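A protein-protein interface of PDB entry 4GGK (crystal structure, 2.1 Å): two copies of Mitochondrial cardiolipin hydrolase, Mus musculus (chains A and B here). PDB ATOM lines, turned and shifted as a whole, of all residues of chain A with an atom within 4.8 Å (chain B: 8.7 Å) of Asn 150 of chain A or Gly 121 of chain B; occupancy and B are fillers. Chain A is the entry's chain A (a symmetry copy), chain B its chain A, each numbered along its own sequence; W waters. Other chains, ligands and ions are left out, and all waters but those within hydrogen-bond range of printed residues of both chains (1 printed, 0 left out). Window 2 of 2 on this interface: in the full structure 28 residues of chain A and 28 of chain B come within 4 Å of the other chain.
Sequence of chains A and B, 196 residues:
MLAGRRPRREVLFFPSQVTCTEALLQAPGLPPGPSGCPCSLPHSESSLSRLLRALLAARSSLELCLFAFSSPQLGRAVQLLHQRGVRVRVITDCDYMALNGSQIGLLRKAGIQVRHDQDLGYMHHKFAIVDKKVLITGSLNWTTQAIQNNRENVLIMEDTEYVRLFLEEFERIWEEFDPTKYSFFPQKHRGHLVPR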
ATOM      1  N   PHE A  14     -27.110 -16.627   5.316  1.00  0.00           N
ATOM      2  CA  PHE A  14     -26.246 -15.757   6.118  1.00  0.00           C
ATOM      3  C   PHE A  14     -25.905 -14.491   5.342  1.00  0.00           C
ATOM      4  O   PHE A  14     -25.935 -14.514   4.129  1.00  0.00           O
ATOM      5  CB  PHE A  14     -24.967 -16.502   6.490  1.00  0.00           C
ATOM      6  CG  PHE A  14     -25.202 -17.644   7.397  1.00  0.00           C
ATOM      7  CD1 PHE A  14     -25.679 -18.857   6.898  1.00  0.00           C
ATOM      8  CD2 PHE A  14     -24.980 -17.521   8.754  1.00  0.00           C
ATOM      9  CE1 PHE A  14     -25.946 -19.928   7.734  1.00  0.00           C
ATOM     10  CE2 PHE A  14     -25.232 -18.607   9.616  1.00  0.00           C
ATOM     11  CZ  PHE A  14     -25.717 -19.813   9.092  1.00  0.00           C
ATOM     12  N   PRO A  15     -25.522 -13.391   6.034  1.00  0.00           N
ATOM     13  CA  PRO A  15     -25.152 -13.234   7.451  1.00  0.00           C
ATOM     14  C   PRO A  15     -26.276 -13.510   8.448  1.00  0.00           C
ATOM     15  O   PRO A  15     -27.435 -13.151   8.189  1.00  0.00           O
ATOM     16  CB  PRO A  15     -24.758 -11.747   7.571  1.00  0.00           C
ATOM     17  CG  PRO A  15     -24.752 -11.199   6.214  1.00  0.00           C
ATOM     18  CD  PRO A  15     -25.504 -12.110   5.316  1.00  0.00           C
ATOM     19  N   GLN A 145     -16.430 -14.653  11.821  1.00  0.00           N
ATOM     20  CA  GLN A 145     -16.315 -13.753  10.680  1.00  0.00           C
ATOM     21  C   GLN A 145     -17.356 -14.070   9.624  1.00  0.00           C
ATOM     22  O   GLN A 145     -18.131 -13.199   9.262  1.00  0.00           O
ATOM     23  CB  GLN A 145     -14.910 -13.808  10.051  1.00  0.00           C
ATOM     24  CG  GLN A 145     -14.702 -12.836   8.875  1.00  0.00           C
ATOM     25  CD  GLN A 145     -14.986 -11.385   9.240  1.00  0.00           C
ATOM     26  OE1 GLN A 145     -14.662 -10.941  10.338  1.00  0.00           O
ATOM     27  NE2 GLN A 145     -15.584 -10.630   8.310  1.00  0.00           N
ATOM     28  N   ALA A 146     -17.391 -15.317   9.151  1.00  0.00           N
ATOM     29  CA  ALA A 146     -18.246 -15.685   8.018  1.00  0.00           C
ATOM     30  C   ALA A 146     -19.716 -15.688   8.394  1.00  0.00           C
ATOM     31  O   ALA A 146     -20.551 -15.153   7.678  1.00  0.00           O
ATOM     32  CB  ALA A 146     -17.823 -17.057   7.424  1.00  0.00           C
ATOM     33  N   GLN A 148     -21.233 -13.892  10.655  1.00  0.00           N
ATOM     34  CA  GLN A 148     -21.789 -12.588  10.929  1.00  0.00           C
ATOM     35  C   GLN A 148     -21.725 -11.628   9.754  1.00  0.00           C
ATOM     36  O   GLN A 148     -22.475 -10.659   9.742  1.00  0.00           O
ATOM     37  CB  GLN A 148     -21.119 -11.976  12.155  1.00  0.00           C
ATOM     38  CG  GLN A 148     -21.494 -12.668  13.472  1.00  0.00           C
ATOM     39  CD  GLN A 148     -22.994 -12.870  13.612  1.00  0.00           C
ATOM     40  OE1 GLN A 148     -23.795 -11.945  13.377  1.00  0.00           O
ATOM     41  NE2 GLN A 148     -23.394 -14.097  13.955  1.00  0.00           N
ATOM     42  N   ASN A 149     -20.861 -11.907   8.773  1.00  0.00           N
ATOM     43  CA  ASN A 149     -20.576 -10.962   7.687  1.00  0.00           C
ATOM     44  C   ASN A 149     -20.746 -11.477   6.241  1.00  0.00           C
ATOM     45  O   ASN A 149     -20.974 -10.683   5.342  1.00  0.00           O
ATOM     46  CB  ASN A 149     -19.160 -10.383   7.841  1.00  0.00           C
ATOM     47  CG  ASN A 149     -18.956  -9.671   9.170  1.00  0.00           C
ATOM     48  OD1 ASN A 149     -19.309  -8.507   9.317  1.00  0.00           O
ATOM     49  ND2 ASN A 149     -18.399 -10.377  10.146  1.00  0.00           N
ATOM     50  N   ASN A 150     -20.620 -12.775   6.009  1.00  0.00           N
ATOM     51  CA  ASN A 150     -20.690 -13.303   4.643  1.00  0.00           C
ATOM     52  C   ASN A 150     -22.068 -13.755   4.201  1.00  0.00           C
ATOM     53  O   ASN A 150     -22.839 -14.302   4.974  1.00  0.00           O
ATOM     54  CB  ASN A 150     -19.768 -14.491   4.483  1.00  0.00           C
ATOM     55  CG  ASN A 150     -18.305 -14.134   4.614  1.00  0.00           C
ATOM     56  OD1 ASN A 150     -17.946 -12.975   4.765  1.00  0.00           O
ATOM     57  ND2 ASN A 150     -17.447 -15.158   4.553  1.00  0.00           N
ATOM     58  N   ARG A 151     -22.343 -13.567   2.923  1.00  0.00           N
ATOM     59  CA  ARG A 151     -23.468 -14.228   2.269  1.00  0.00           C
ATOM     60  C   ARG A 151     -23.123 -15.692   2.049  1.00  0.00           C
ATOM     61  O   ARG A 151     -22.172 -16.002   1.325  1.00  0.00           O
ATOM     62  CB  ARG A 151     -23.793 -13.546   0.940  1.00  0.00           C
ATOM     63  CG  ARG A 151     -23.714 -12.038   1.065  1.00  0.00           C
ATOM     64  CD  ARG A 151     -24.568 -11.322   0.095  1.00  0.00           C
ATOM     65  NE  ARG A 151     -24.225  -9.907   0.178  1.00  0.00           N
ATOM     66  CZ  ARG A 151     -25.093  -8.906   0.178  1.00  0.00           C
ATOM     67  NH1 ARG A 151     -26.407  -9.125   0.109  1.00  0.00           N
ATOM     68  NH2 ARG A 151     -24.625  -7.666   0.270  1.00  0.00           N
ATOM     69  N   GLU A 152     -23.884 -16.564   2.711  1.00  0.00           N
ATOM     70  CA  GLU A 152     -23.673 -18.003   2.704  1.00  0.00           C
ATOM     71  C   GLU A 152     -25.015 -18.746   2.730  1.00  0.00           C
ATOM     72  O   GLU A 152     -26.054 -18.177   3.068  1.00  0.00           O
ATOM     73  CB  GLU A 152     -22.884 -18.415   3.947  1.00  0.00           C
ATOM     74  CG  GLU A 152     -21.665 -17.565   4.276  1.00  0.00           C
ATOM     75  CD  GLU A 152     -20.359 -18.145   3.737  1.00  0.00           C
ATOM     76  OE1 GLU A 152     -20.374 -19.050   2.890  1.00  0.00           O
ATOM     77  OE2 GLU A 152     -19.305 -17.655   4.140  1.00  0.00           O
ATOM     78  N   PHE B  67     -18.503 -17.134  -5.397  1.00  0.00           N
ATOM     79  CA  PHE B  67     -17.373 -16.496  -4.767  1.00  0.00           C
ATOM     80  C   PHE B  67     -16.214 -16.276  -5.778  1.00  0.00           C
ATOM     81  O   PHE B  67     -15.700 -15.148  -5.885  1.00  0.00           O
ATOM     82  CB  PHE B  67     -16.919 -17.316  -3.547  1.00  0.00           C
ATOM     83  CG  PHE B  67     -15.694 -16.773  -2.871  1.00  0.00           C
ATOM     84  CD1 PHE B  67     -15.691 -15.504  -2.332  1.00  0.00           C
ATOM     85  CD2 PHE B  67     -14.534 -17.539  -2.795  1.00  0.00           C
ATOM     86  CE1 PHE B  67     -14.566 -14.991  -1.733  1.00  0.00           C
ATOM     87  CE2 PHE B  67     -13.397 -17.043  -2.197  1.00  0.00           C
ATOM     88  CZ  PHE B  67     -13.408 -15.754  -1.660  1.00  0.00           C
ATOM     89  N   THR B  92     -20.454 -12.333  -8.573  1.00  0.00           N
ATOM     90  CA  THR B  92     -19.198 -12.819  -7.981  1.00  0.00           C
ATOM     91  C   THR B  92     -18.691 -11.922  -6.863  1.00  0.00           C
ATOM     92  O   THR B  92     -19.159 -10.800  -6.695  1.00  0.00           O
ATOM     93  CB  THR B  92     -18.049 -12.926  -8.996  1.00  0.00           C
ATOM     94  OG1 THR B  92     -17.867 -11.651  -9.664  1.00  0.00           O
ATOM     95  CG2 THR B  92     -18.301 -14.037  -9.986  1.00  0.00           C
ATOM     96  N   ASP B  93     -17.723 -12.414  -6.092  1.00  0.00           N
ATOM     97  CA  ASP B  93     -17.186 -11.619  -4.964  1.00  0.00           C
ATOM     98  C   ASP B  93     -16.245 -10.532  -5.417  1.00  0.00           C
ATOM     99  O   ASP B  93     -16.217  -9.436  -4.838  1.00  0.00           O
ATOM    100  CB  ASP B  93     -16.424 -12.458  -3.941  1.00  0.00           C
ATOM    101  CG  ASP B  93     -16.038 -11.644  -2.712  1.00  0.00           C
ATOM    102  OD1 ASP B  93     -16.954 -11.226  -2.000  1.00  0.00           O
ATOM    103  OD2 ASP B  93     -14.842 -11.383  -2.468  1.00  0.00           O
ATOM    104  N   CYS B  94     -15.405 -10.857  -6.390  1.00  0.00           N
ATOM    105  CA  CYS B  94     -14.389  -9.916  -6.796  1.00  0.00           C
ATOM    106  C   CYS B  94     -14.725  -9.410  -8.185  1.00  0.00           C
ATOM    107  O   CYS B  94     -15.367 -10.121  -8.965  1.00  0.00           O
ATOM    108  CB  CYS B  94     -13.004 -10.562  -6.734  1.00  0.00           C
ATOM    109  SG  CYS B  94     -12.744 -11.814  -7.946  1.00  0.00           S
ATOM    110  N   ASP B 117     -19.240  -8.002  -5.446  1.00  0.00           N
ATOM    111  CA  ASP B 117     -18.920  -7.618  -4.051  1.00  0.00           C
ATOM    112  C   ASP B 117     -17.584  -6.823  -3.961  1.00  0.00           C
ATOM    113  O   ASP B 117     -17.006  -6.431  -4.997  1.00  0.00           O
ATOM    114  CB  ASP B 117     -18.858  -8.889  -3.182  1.00  0.00           C
ATOM    115  CG  ASP B 117     -19.248  -8.644  -1.697  1.00  0.00           C
ATOM    116  OD1 ASP B 117     -20.453  -8.699  -1.322  1.00  0.00           O
ATOM    117  OD2 ASP B 117     -18.330  -8.444  -0.892  1.00  0.00           O
ATOM    118  N   GLN B 118     -17.091  -6.601  -2.734  1.00  0.00           N
ATOM    119  CA  GLN B 118     -15.919  -5.742  -2.492  1.00  0.00           C
ATOM    120  C   GLN B 118     -14.566  -6.505  -2.541  1.00  0.00           C
ATOM    121  O   GLN B 118     -13.562  -6.042  -1.995  1.00  0.00           O
ATOM    122  CB  GLN B 118     -16.083  -5.006  -1.137  1.00  0.00           C
ATOM    123  CG  GLN B 118     -17.210  -3.938  -1.059  1.00  0.00           C
ATOM    124  CD  GLN B 118     -17.159  -2.894  -2.191  1.00  0.00           C
ATOM    125  OE1 GLN B 118     -17.733  -3.103  -3.266  1.00  0.00           O
ATOM    126  NE2 GLN B 118     -16.492  -1.761  -1.937  1.00  0.00           N
ATOM    127  N   ASP B 119     -14.534  -7.655  -3.216  1.00  0.00           N
ATOM    128  CA  ASP B 119     -13.391  -8.598  -3.145  1.00  0.00           C
ATOM    129  C   ASP B 119     -12.822  -8.765  -1.702  1.00  0.00           C
ATOM    130  O   ASP B 119     -11.600  -8.917  -1.522  1.00  0.00           O
ATOM    131  CB  ASP B 119     -12.269  -8.189  -4.129  1.00  0.00           C
ATOM    132  CG  ASP B 119     -11.117  -9.215  -4.181  1.00  0.00           C
ATOM    133  OD1 ASP B 119     -11.412 -10.409  -4.096  1.00  0.00           O
ATOM    134  OD2 ASP B 119      -9.924  -8.835  -4.285  1.00  0.00           O
ATOM    135  N   LEU B 120     -13.701  -8.711  -0.687  1.00  0.00           N
ATOM    136  CA  LEU B 120     -13.298  -8.819   0.732  1.00  0.00           C
ATOM    137  C   LEU B 120     -13.658 -10.186   1.344  1.00  0.00           C
ATOM    138  O   LEU B 120     -13.405 -10.427   2.529  1.00  0.00           O
ATOM    139  CB  LEU B 120     -13.940  -7.699   1.563  1.00  0.00           C
ATOM    140  CG  LEU B 120     -13.245  -6.328   1.532  1.00  0.00           C
ATOM    141  CD1 LEU B 120     -13.957  -5.384   2.479  1.00  0.00           C
ATOM    142  CD2 LEU B 120     -11.767  -6.450   1.876  1.00  0.00           C
ATOM    143  N   GLY B 121     -14.252 -11.066   0.543  1.00  0.00           N
ATOM    144  CA  GLY B 121     -14.696 -12.379   1.022  1.00  0.00           C
ATOM    145  C   GLY B 121     -16.188 -12.483   1.284  1.00  0.00           C
ATOM    146  O   GLY B 121     -16.708 -13.601   1.417  1.00  0.00           O
ATOM    147  N   TYR B 122     -16.888 -11.343   1.329  1.00  0.00           N
ATOM    148  CA  TYR B 122     -18.281 -11.325   1.780  1.00  0.00           C
ATOM    149  C   TYR B 122     -19.255 -12.150   0.924  1.00  0.00           C
ATOM    150  O   TYR B 122     -20.150 -12.743   1.491  1.00  0.00           O
ATOM    151  CB  TYR B 122     -18.830  -9.901   1.936  1.00  0.00           C
ATOM    152  CG  TYR B 122     -18.047  -8.996   2.880  1.00  0.00           C
ATOM    153  CD1 TYR B 122     -17.538  -9.465   4.091  1.00  0.00           C
ATOM    154  CD2 TYR B 122     -17.844  -7.658   2.562  1.00  0.00           C
ATOM    155  CE1 TYR B 122     -16.830  -8.620   4.953  1.00  0.00           C
ATOM    156  CE2 TYR B 122     -17.152  -6.819   3.399  1.00  0.00           C
ATOM    157  CZ  TYR B 122     -16.637  -7.299   4.598  1.00  0.00           C
ATOM    158  OH  TYR B 122     -15.946  -6.447   5.434  1.00  0.00           O
ATOM    159  N   MET B 123     -19.108 -12.193  -0.403  1.00  0.00           N
ATOM    160  CA  MET B 123     -20.089 -12.895  -1.240  1.00  0.00           C
ATOM    161  C   MET B 123     -19.568 -14.296  -1.514  1.00  0.00           C
ATOM    162  O   MET B 123     -18.823 -14.513  -2.483  1.00  0.00           O
ATOM    163  CB  MET B 123     -20.343 -12.146  -2.555  1.00  0.00           C
ATOM    164  CG  MET B 123     -21.733 -12.344  -3.140  1.00  0.00           C
ATOM    165  SD  MET B 123     -22.287 -14.040  -3.402  1.00  0.00           S
ATOM    166  CE  MET B 123     -21.180 -14.666  -4.641  1.00  0.00           C
ATOM    167  N   HIS B 124     -19.959 -15.232  -0.648  1.00  0.00           N
ATOM    168  CA  HIS B 124     -19.278 -16.518  -0.510  1.00  0.00           C
ATOM    169  C   HIS B 124     -20.102 -17.737  -1.037  1.00  0.00           C
ATOM    170  O   HIS B 124     -19.613 -18.859  -1.019  1.00  0.00           O
ATOM    171  CB  HIS B 124     -18.830 -16.734   0.948  1.00  0.00           C
ATOM    172  CG  HIS B 124     -17.784 -17.811   1.121  1.00  0.00           C
ATOM    173  ND1 HIS B 124     -18.086 -19.103   1.512  1.00  0.00           N
ATOM    174  CD2 HIS B 124     -16.435 -17.781   0.959  1.00  0.00           C
ATOM    175  CE1 HIS B 124     -16.982 -19.827   1.563  1.00  0.00           C
ATOM    176  NE2 HIS B 124     -15.960 -19.048   1.253  1.00  0.00           N
ATOM    177  N   HIS B 125     -21.318 -17.509  -1.523  1.00  0.00           N
ATOM    178  CA  HIS B 125     -22.085 -18.558  -2.206  1.00  0.00           C
ATOM    179  C   HIS B 125     -21.320 -19.221  -3.361  1.00  0.00           C
ATOM    180  O   HIS B 125     -20.464 -18.592  -3.987  1.00  0.00           O
ATOM    181  CB  HIS B 125     -23.380 -18.018  -2.789  1.00  0.00           C
ATOM    182  CG  HIS B 125     -24.382 -17.512  -1.788  1.00  0.00           C
ATOM    183  ND1 HIS B 125     -24.999 -18.325  -0.867  1.00  0.00           N
ATOM    184  CD2 HIS B 125     -24.931 -16.286  -1.630  1.00  0.00           C
ATOM    185  CE1 HIS B 125     -25.858 -17.619  -0.161  1.00  0.00           C
ATOM    186  NE2 HIS B 125     -25.837 -16.375  -0.607  1.00  0.00           N
ATOM    187  N   LYS B 126     -21.664 -20.485  -3.648  1.00  0.00           N
ATOM    188  CA  LYS B 126     -21.232 -21.170  -4.852  1.00  0.00           C
ATOM    189  C   LYS B 126     -22.389 -21.931  -5.499  1.00  0.00           C
ATOM    190  O   LYS B 126     -22.415 -23.169  -5.490  1.00  0.00           O
ATOM    191  CB  LYS B 126     -20.052 -22.124  -4.590  1.00  0.00           C
ATOM    192  CG  LYS B 126     -18.875 -21.554  -3.740  1.00  0.00           C
ATOM    193  CD  LYS B 126     -19.048 -21.920  -2.285  1.00  0.00           C
ATOM    194  CE  LYS B 126     -17.751 -21.775  -1.478  1.00  0.00           C
ATOM    195  NZ  LYS B 126     -17.218 -20.431  -1.588  1.00  0.00           N
ATOM    196  N   GLU B 169     -33.057 -15.267  -2.908  1.00  0.00           N
ATOM    197  CA  GLU B 169     -31.777 -14.764  -2.397  1.00  0.00           C
ATOM    198  C   GLU B 169     -30.984 -14.134  -3.535  1.00  0.00           C
ATOM    199  O   GLU B 169     -30.460 -13.022  -3.392  1.00  0.00           O
ATOM    200  CB  GLU B 169     -30.985 -15.871  -1.696  1.00  0.00           C
ATOM    201  CG  GLU B 169     -29.519 -15.533  -1.354  1.00  0.00           C
ATOM    202  CD  GLU B 169     -29.331 -14.721  -0.068  1.00  0.00           C
ATOM    203  OE1 GLU B 169     -30.272 -14.046   0.394  1.00  0.00           O
ATOM    204  OE2 GLU B 169     -28.204 -14.789   0.493  1.00  0.00           O
ATOM    205  N   ILE B 173     -29.699  -9.985  -3.731  1.00  0.00           N
ATOM    206  CA  ILE B 173     -28.304  -9.633  -3.967  1.00  0.00           C
ATOM    207  C   ILE B 173     -28.155  -8.884  -5.301  1.00  0.00           C
ATOM    208  O   ILE B 173     -27.452  -7.860  -5.353  1.00  0.00           O
ATOM    209  CB  ILE B 173     -27.359 -10.857  -3.909  1.00  0.00           C
ATOM    210  CG1 ILE B 173     -27.508 -11.623  -2.582  1.00  0.00           C
ATOM    211  CG2 ILE B 173     -25.906 -10.404  -4.030  1.00  0.00           C
ATOM    212  CD1 ILE B 173     -26.981 -13.049  -2.633  1.00  0.00           C
HETATM  213  O   HOH W   1     -17.271 -19.132   4.829  1.00  0.00           O
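Gln 145 of chain A touches none of the printed residues of chain B.
No residue of chain B comes within 4 Å of Ala 146 of chain A.
Of the printed residues of chain B, Asn 149 of chain A touches Tyr 122 (3.9 Å).
Asn 150 of chain A touches two residues of chain B.
Of the printed residues of chain B, Arg 151 of chain A touches Tyr 122, His 124, His 125 and Ile 173.
Of the printed residues of chain B, Glu 152 of chain A touches His 124 and His 125.
Gln 118 of chain B touches none of the printed residues of chain A.
Gly 121 of chain B touches just one residue of chain A: Asn 150 (3.6 Å).
Of the printed residues of chain A, His 124 of chain B touches Arg 151 (3.1 Å) and Glu 152 (2.7 Å).
Printed residues of chain A within 4 Å of Ile 173 of chain B: Arg 151.
The nearest residue of chain B that does not touch Asn 150 of chain A is His 124 of chain B (4.2 Å).
The nearest printed residue of chain A that does not touch Gly 121 of chain B is Glu 152 of chain A (5.5 Å).
The nearest printed residue of chain A that does not touch His 124 of chain B is Asn 150 of chain A (4.2 Å).
The backbone NH of His 124 of chain B sits at hydrogen-bond distance from the backbone carbonyl oxygen of Arg 151 of chain A, 3.1 Å away.
The backbone NH (N) of Arg 151 of chain A is in hydrogen-bond range of the backbone carbonyl oxygen (O) of Tyr 122 of chain B (2.7 Å).
The backbone carbonyl oxygen (O) of Arg 151 of chain A sits at hydrogen-bond distance from the backbone NH (N) of His 125 of chain B.
ND1 of His 124 of chain B sits at hydrogen-bond distance from OE1 of Glu 152 of chain A.
Of the 9 printed residues of chain A, 4 touch a printed residue of chain B.
Among the printed residues, no Asp or Glu carboxylate lies within 4 Å of a Lys or Arg side-chain nitrogen of the other chain.
NE2 of His 125 of chain B is in hydrogen-bond range of OE2 of Glu 169 of chain B, at 3.1 Å.
ND2 of Asn 150 of chain A lies within hydrogen-bond range of OE2 of Glu 152 of chain A (3.1 Å).
N of Phe 14 of chain A sits at hydrogen-bond distance from O of Glu 152 of chain A.
N of Tyr 122 of chain B is in hydrogen-bond range of OD1 of Asp 93 of chain B (3.3 Å).
N of Phe 67 of chain B is in hydrogen-bond range of O of His 125 of chain B (2.8 Å).
The backbone carbonyl oxygen of Gln 145 of chain A lies within hydrogen-bond range of the side-chain amide nitrogen of Asn 149 of chain A, at 3.0 Å.
Tyr 122 of chain B touches Asn 149 of chain A (CD1 to O, 3.9 Å).
Asn 150 of chain A touches Gly 121 of chain B.
Tyr 122 of chain B touches Asn 150 of chain A.
Arg 151 of chain A touches Ile 173 of chain B (NH1 to CG1, 3.8 Å).
His 125 of chain B touches Glu 152 of chain A.
Water W1 bridges OE2 of Glu 152 of chain A (2.6 Å) and ND1 of His 124 of chain B (3.4 Å).
No position is printed for both chains.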
